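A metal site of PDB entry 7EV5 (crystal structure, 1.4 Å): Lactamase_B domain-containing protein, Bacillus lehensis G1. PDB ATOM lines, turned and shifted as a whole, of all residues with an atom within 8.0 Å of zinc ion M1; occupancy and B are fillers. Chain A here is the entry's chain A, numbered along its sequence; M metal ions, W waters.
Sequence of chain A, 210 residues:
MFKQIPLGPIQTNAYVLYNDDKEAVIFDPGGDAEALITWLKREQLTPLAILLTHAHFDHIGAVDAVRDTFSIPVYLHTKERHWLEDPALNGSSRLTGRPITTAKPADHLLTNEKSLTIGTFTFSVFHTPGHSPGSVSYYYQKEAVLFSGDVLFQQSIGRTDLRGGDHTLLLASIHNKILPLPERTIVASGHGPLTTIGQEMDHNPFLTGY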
ATOM      1  N   ILE A  10     -29.929  38.861  26.047  1.00  0.00           N
ATOM      2  CA  ILE A  10     -29.148  37.908  26.817  1.00  0.00           C
ATOM      3  C   ILE A  10     -27.658  37.992  26.469  1.00  0.00           C
ATOM      4  O   ILE A  10     -26.804  37.604  27.280  1.00  0.00           O
ATOM      5  CB  ILE A  10     -29.705  36.484  26.632  1.00  0.00           C
ATOM      6  CG1 ILE A  10     -31.219  36.468  26.887  1.00  0.00           C
ATOM      7  CG2 ILE A  10     -28.988  35.470  27.525  1.00  0.00           C
ATOM      8  CD1 ILE A  10     -31.590  36.739  28.330  1.00  0.00           C
ATOM      9  N   GLN A  11     -27.336  38.497  25.274  1.00  0.00           N
ATOM     10  CA  GLN A  11     -25.962  38.623  24.789  1.00  0.00           C
ATOM     11  C   GLN A  11     -25.305  37.272  24.542  1.00  0.00           C
ATOM     12  O   GLN A  11     -24.081  37.146  24.620  1.00  0.00           O
ATOM     13  CB  GLN A  11     -25.101  39.534  25.667  1.00  0.00           C
ATOM     14  CG  GLN A  11     -25.485  41.001  25.585  1.00  0.00           C
ATOM     15  CD  GLN A  11     -25.013  41.646  24.286  1.00  0.00           C
ATOM     16  OE1 GLN A  11     -23.845  41.982  24.143  1.00  0.00           O
ATOM     17  NE2 GLN A  11     -25.933  41.809  23.342  1.00  0.00           N
ATOM     18  N   THR A  12     -26.122  36.259  24.235  1.00  0.00           N
ATOM     19  CA  THR A  12     -25.605  34.957  23.839  1.00  0.00           C
ATOM     20  C   THR A  12     -24.676  35.096  22.649  1.00  0.00           C
ATOM     21  O   THR A  12     -24.953  35.846  21.700  1.00  0.00           O
ATOM     22  CB  THR A  12     -26.786  34.076  23.455  1.00  0.00           C
ATOM     23  OG1 THR A  12     -27.669  33.973  24.589  1.00  0.00           O
ATOM     24  CG2 THR A  12     -26.338  32.659  23.063  1.00  0.00           C
ATOM     25  N   ASN A  13     -23.573  34.358  22.689  1.00  0.00           N
ATOM     26  CA  ASN A  13     -22.561  34.433  21.625  1.00  0.00           C
ATOM     27  C   ASN A  13     -23.023  33.600  20.436  1.00  0.00           C
ATOM     28  O   ASN A  13     -23.059  32.367  20.500  1.00  0.00           O
ATOM     29  CB  ASN A  13     -21.234  33.869  22.121  1.00  0.00           C
ATOM     30  CG  ASN A  13     -20.621  34.695  23.215  1.00  0.00           C
ATOM     31  OD1 ASN A  13     -20.603  35.922  23.135  1.00  0.00           O
ATOM     32  ND2 ASN A  13     -20.098  34.038  24.235  1.00  0.00           N
ATOM     33  N   ASP A  28     -25.519  29.336  16.380  1.00  0.00           N
ATOM     34  CA  ASP A  28     -26.350  29.916  17.422  1.00  0.00           C
ATOM     35  C   ASP A  28     -26.725  31.388  17.211  1.00  0.00           C
ATOM     36  O   ASP A  28     -26.390  32.239  18.042  1.00  0.00           O
ATOM     37  CB  ASP A  28     -25.698  29.743  18.796  1.00  0.00           C
ATOM     38  CG  ASP A  28     -25.595  28.288  19.220  1.00  0.00           C
ATOM     39  OD1 ASP A  28     -25.959  27.384  18.447  1.00  0.00           O
ATOM     40  OD2 ASP A  28     -25.120  28.047  20.352  1.00  0.00           O
ATOM     41  N   THR A  53     -25.894  24.583  18.608  1.00  0.00           N
ATOM     42  CA  THR A  53     -25.429  23.758  19.709  1.00  0.00           C
ATOM     43  C   THR A  53     -26.598  23.178  20.480  1.00  0.00           C
ATOM     44  O   THR A  53     -26.523  22.038  20.980  1.00  0.00           O
ATOM     45  CB  THR A  53     -24.506  24.546  20.651  1.00  0.00           C
ATOM     46  OG1 THR A  53     -25.243  25.589  21.305  1.00  0.00           O
ATOM     47  CG2 THR A  53     -23.326  25.123  19.909  1.00  0.00           C
ATOM     48  N   HIS A  54     -27.676  23.945  20.604  1.00  0.00           N
ATOM     49  CA  HIS A  54     -28.906  23.539  21.272  1.00  0.00           C
ATOM     50  C   HIS A  54     -29.982  24.564  20.937  1.00  0.00           C
ATOM     51  O   HIS A  54     -29.707  25.592  20.308  1.00  0.00           O
ATOM     52  CB  HIS A  54     -28.727  23.295  22.782  1.00  0.00           C
ATOM     53  CG  HIS A  54     -28.406  24.518  23.615  1.00  0.00           C
ATOM     54  ND1 HIS A  54     -27.318  25.327  23.389  1.00  0.00           N
ATOM     55  CD2 HIS A  54     -29.000  24.985  24.737  1.00  0.00           C
ATOM     56  CE1 HIS A  54     -27.271  26.271  24.326  1.00  0.00           C
ATOM     57  NE2 HIS A  54     -28.281  26.094  25.148  1.00  0.00           N
ATOM     58  N   HIS A  56     -32.265  26.200  23.071  1.00  0.00           N
ATOM     59  CA  HIS A  56     -32.770  27.210  23.993  1.00  0.00           C
ATOM     60  C   HIS A  56     -33.043  28.509  23.244  1.00  0.00           C
ATOM     61  O   HIS A  56     -32.338  28.861  22.287  1.00  0.00           O
ATOM     62  CB  HIS A  56     -31.770  27.467  25.121  1.00  0.00           C
ATOM     63  CG  HIS A  56     -31.849  26.465  26.226  1.00  0.00           C
ATOM     64  ND1 HIS A  56     -30.767  26.173  27.029  1.00  0.00           N
ATOM     65  CD2 HIS A  56     -32.863  25.702  26.674  1.00  0.00           C
ATOM     66  CE1 HIS A  56     -31.114  25.270  27.926  1.00  0.00           C
ATOM     67  NE2 HIS A  56     -32.387  24.967  27.726  1.00  0.00           N
ATOM     68  N   PHE A  57     -34.054  29.244  23.724  1.00  0.00           N
ATOM     69  CA  PHE A  57     -34.527  30.428  23.015  1.00  0.00           C
ATOM     70  C   PHE A  57     -33.409  31.435  22.730  1.00  0.00           C
ATOM     71  O   PHE A  57     -33.431  32.125  21.710  1.00  0.00           O
ATOM     72  CB  PHE A  57     -35.649  31.102  23.825  1.00  0.00           C
ATOM     73  CG  PHE A  57     -35.152  31.811  25.067  1.00  0.00           C
ATOM     74  CD1 PHE A  57     -34.886  33.184  25.051  1.00  0.00           C
ATOM     75  CD2 PHE A  57     -34.942  31.109  26.244  1.00  0.00           C
ATOM     76  CE1 PHE A  57     -34.415  33.824  26.190  1.00  0.00           C
ATOM     77  CE2 PHE A  57     -34.475  31.740  27.384  1.00  0.00           C
ATOM     78  CZ  PHE A  57     -34.205  33.101  27.355  1.00  0.00           C
ATOM     79  N   ASP A  58     -32.438  31.569  23.646  1.00  0.00           N
ATOM     80  CA  ASP A  58     -31.403  32.574  23.496  1.00  0.00           C
ATOM     81  C   ASP A  58     -30.386  32.219  22.429  1.00  0.00           C
ATOM     82  O   ASP A  58     -29.527  33.043  22.113  1.00  0.00           O
ATOM     83  CB  ASP A  58     -30.736  32.856  24.847  1.00  0.00           C
ATOM     84  CG  ASP A  58     -30.087  31.626  25.471  1.00  0.00           C
ATOM     85  OD1 ASP A  58     -30.809  30.620  25.684  1.00  0.00           O
ATOM     86  OD2 ASP A  58     -28.862  31.684  25.754  1.00  0.00           O
ATOM     87  N   HIS A  59     -30.493  31.021  21.852  1.00  0.00           N
ATOM     88  CA  HIS A  59     -29.618  30.593  20.764  1.00  0.00           C
ATOM     89  C   HIS A  59     -30.311  30.539  19.419  1.00  0.00           C
ATOM     90  O   HIS A  59     -29.649  30.253  18.415  1.00  0.00           O
ATOM     91  CB  HIS A  59     -28.984  29.234  21.097  1.00  0.00           C
ATOM     92  CG  HIS A  59     -28.137  29.268  22.335  1.00  0.00           C
ATOM     93  ND1 HIS A  59     -26.765  29.157  22.321  1.00  0.00           N
ATOM     94  CD2 HIS A  59     -28.481  29.485  23.627  1.00  0.00           C
ATOM     95  CE1 HIS A  59     -26.302  29.289  23.550  1.00  0.00           C
ATOM     96  NE2 HIS A  59     -27.324  29.503  24.364  1.00  0.00           N
ATOM     97  N   HIS A 131     -26.617  20.307  30.178  1.00  0.00           N
ATOM     98  CA  HIS A 131     -27.339  21.578  30.166  1.00  0.00           C
ATOM     99  C   HIS A 131     -28.651  21.448  29.377  1.00  0.00           C
ATOM    100  O   HIS A 131     -29.668  22.036  29.763  1.00  0.00           O
ATOM    101  CB  HIS A 131     -26.430  22.673  29.599  1.00  0.00           C
ATOM    102  CG  HIS A 131     -27.126  23.958  29.282  1.00  0.00           C
ATOM    103  ND1 HIS A 131     -27.428  24.906  30.234  1.00  0.00           N
ATOM    104  CD2 HIS A 131     -27.535  24.470  28.094  1.00  0.00           C
ATOM    105  CE1 HIS A 131     -28.009  25.949  29.657  1.00  0.00           C
ATOM    106  NE2 HIS A 131     -28.093  25.697  28.351  1.00  0.00           N
ATOM    107  N   GLY A 149     -21.388  25.507  22.835  1.00  0.00           N
ATOM    108  CA  GLY A 149     -22.615  25.967  23.452  1.00  0.00           C
ATOM    109  C   GLY A 149     -22.445  26.239  24.942  1.00  0.00           C
ATOM    110  O   GLY A 149     -21.497  26.890  25.377  1.00  0.00           O
ATOM    111  N   ASP A 150     -23.394  25.728  25.738  1.00  0.00           N
ATOM    112  CA  ASP A 150     -23.501  26.105  27.141  1.00  0.00           C
ATOM    113  C   ASP A 150     -22.996  25.033  28.081  1.00  0.00           C
ATOM    114  O   ASP A 150     -23.445  24.953  29.226  1.00  0.00           O
ATOM    115  CB  ASP A 150     -24.937  26.517  27.477  1.00  0.00           C
ATOM    116  CG  ASP A 150     -25.367  27.815  26.814  1.00  0.00           C
ATOM    117  OD1 ASP A 150     -24.566  28.393  26.043  1.00  0.00           O
ATOM    118  OD2 ASP A 150     -26.513  28.239  27.051  1.00  0.00           O
ATOM    119  N   VAL A 151     -22.043  24.212  27.636  1.00  0.00           N
ATOM    120  CA  VAL A 151     -21.498  23.178  28.502  1.00  0.00           C
ATOM    121  C   VAL A 151     -20.435  23.744  29.442  1.00  0.00           C
ATOM    122  O   VAL A 151     -20.468  23.527  30.656  1.00  0.00           O
ATOM    123  CB  VAL A 151     -20.945  22.040  27.639  1.00  0.00           C
ATOM    124  CG1 VAL A 151     -20.190  21.033  28.477  1.00  0.00           C
ATOM    125  CG2 VAL A 151     -22.087  21.346  26.897  1.00  0.00           C
ATOM    126  N   PHE A 153     -17.927  27.223  30.293  1.00  0.00           N
ATOM    127  CA  PHE A 153     -17.647  28.639  30.095  1.00  0.00           C
ATOM    128  C   PHE A 153     -16.304  28.952  30.718  1.00  0.00           C
ATOM    129  O   PHE A 153     -15.698  28.135  31.410  1.00  0.00           O
ATOM    130  CB  PHE A 153     -18.703  29.509  30.792  1.00  0.00           C
ATOM    131  CG  PHE A 153     -20.122  29.183  30.396  1.00  0.00           C
ATOM    132  CD1 PHE A 153     -20.556  29.343  29.084  1.00  0.00           C
ATOM    133  CD2 PHE A 153     -21.041  28.761  31.348  1.00  0.00           C
ATOM    134  CE1 PHE A 153     -21.875  29.071  28.732  1.00  0.00           C
ATOM    135  CE2 PHE A 153     -22.363  28.480  30.996  1.00  0.00           C
ATOM    136  CZ  PHE A 153     -22.781  28.625  29.678  1.00  0.00           C
ATOM    137  N   ARG A 159     -25.608  25.856  33.404  1.00  0.00           N
ATOM    138  CA  ARG A 159     -26.644  25.587  34.387  1.00  0.00           C
ATOM    139  C   ARG A 159     -27.345  24.287  34.039  1.00  0.00           C
ATOM    140  O   ARG A 159     -27.504  23.926  32.867  1.00  0.00           O
ATOM    141  CB  ARG A 159     -27.647  26.748  34.463  1.00  0.00           C
ATOM    142  CG  ARG A 159     -28.448  26.992  33.198  1.00  0.00           C
ATOM    143  CD  ARG A 159     -29.136  28.347  33.234  1.00  0.00           C
ATOM    144  NE  ARG A 159     -30.183  28.397  34.245  1.00  0.00           N
ATOM    145  CZ  ARG A 159     -31.011  29.423  34.430  1.00  0.00           C
ATOM    146  NH1 ARG A 159     -30.914  30.523  33.677  1.00  0.00           N
ATOM    147  NH2 ARG A 159     -31.931  29.347  35.378  1.00  0.00           N
ATOM    148  N   LEU A 162     -32.554  23.605  33.997  1.00  0.00           N
ATOM    149  CA  LEU A 162     -33.584  23.811  32.990  1.00  0.00           C
ATOM    150  C   LEU A 162     -34.167  22.470  32.513  1.00  0.00           C
ATOM    151  O   LEU A 162     -33.885  21.415  33.075  1.00  0.00           O
ATOM    152  CB  LEU A 162     -33.052  24.714  31.870  1.00  0.00           C
ATOM    153  CG  LEU A 162     -32.412  26.037  32.304  1.00  0.00           C
ATOM    154  CD1 LEU A 162     -31.906  26.851  31.101  1.00  0.00           C
ATOM    155  CD2 LEU A 162     -33.377  26.851  33.146  1.00  0.00           C
ATOM    156  N   SER A 189     -17.910  29.374  23.626  1.00  0.00           N
ATOM    157  CA  SER A 189     -19.108  28.991  24.358  1.00  0.00           C
ATOM    158  C   SER A 189     -20.229  30.002  24.155  1.00  0.00           C
ATOM    159  O   SER A 189     -20.069  31.045  23.535  1.00  0.00           O
ATOM    160  CB  SER A 189     -18.782  28.848  25.847  1.00  0.00           C
ATOM    161  OG  SER A 189     -18.573  30.120  26.426  1.00  0.00           O
ATOM    162  N   GLY A 190     -21.397  29.646  24.678  1.00  0.00           N
ATOM    163  CA  GLY A 190     -22.586  30.447  24.440  1.00  0.00           C
ATOM    164  C   GLY A 190     -22.649  31.725  25.240  1.00  0.00           C
ATOM    165  O   GLY A 190     -23.443  32.600  24.893  1.00  0.00           O
ATOM    166  N   HIS A 191     -21.858  31.856  26.304  1.00  0.00           N
ATOM    167  CA  HIS A 191     -21.997  33.023  27.175  1.00  0.00           C
ATOM    168  C   HIS A 191     -20.626  33.410  27.719  1.00  0.00           C
ATOM    169  O   HIS A 191     -19.904  32.551  28.220  1.00  0.00           O
ATOM    170  CB  HIS A 191     -22.963  32.706  28.331  1.00  0.00           C
ATOM    171  CG  HIS A 191     -24.339  32.323  27.863  1.00  0.00           C
ATOM    172  ND1 HIS A 191     -25.333  33.252  27.620  1.00  0.00           N
ATOM    173  CD2 HIS A 191     -24.879  31.120  27.562  1.00  0.00           C
ATOM    174  CE1 HIS A 191     -26.413  32.632  27.191  1.00  0.00           C
ATOM    175  NE2 HIS A 191     -26.166  31.339  27.142  1.00  0.00           N
HETATM  176 ZN    ZN M   1     -27.423  29.947  26.363  1.00  0.00          ZN
HETATM  177 ZN    ZN M   2     -28.820  26.992  26.921  1.00  0.00          ZN
HETATM  178  O   HOH W   1     -29.028  28.922  26.974  1.00  0.00           O
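Zinc ion M1 is bound by water W1. A ring nitrogen (NE2) of His 191 is bound to zinc ion M1 (2.0 Å). Zinc ion M1 is bound by NE2 of His 59. Zinc ion M1 is bound by OD2 of Asp 150 (2.1 Å). Zinc ion M1 is bound by OD2 of Asp 58, at 2.3 Å.
The backbone NH (N) of His 191 lies close to the side-chain amide nitrogen (ND2) of Asn 13, 3.5 Å away. The side-chain hydroxyl (OG) of Ser 189 is in hydrogen-bond range of the backbone carbonyl oxygen (O) of His 191 (3.3 Å). A ring nitrogen (ND1) of His 59 sits at hydrogen-bond distance from the side-chain carboxylate (OD2) of Asp 28 (2.8 Å). O of Asp 58 sits close to OG1 of Thr 12.
Of the 21 residues printed, 4 come within 4 Å of zinc ion M1. Along chain A the residues within 4 Å of zinc ion M1 span positions 58 to 191.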
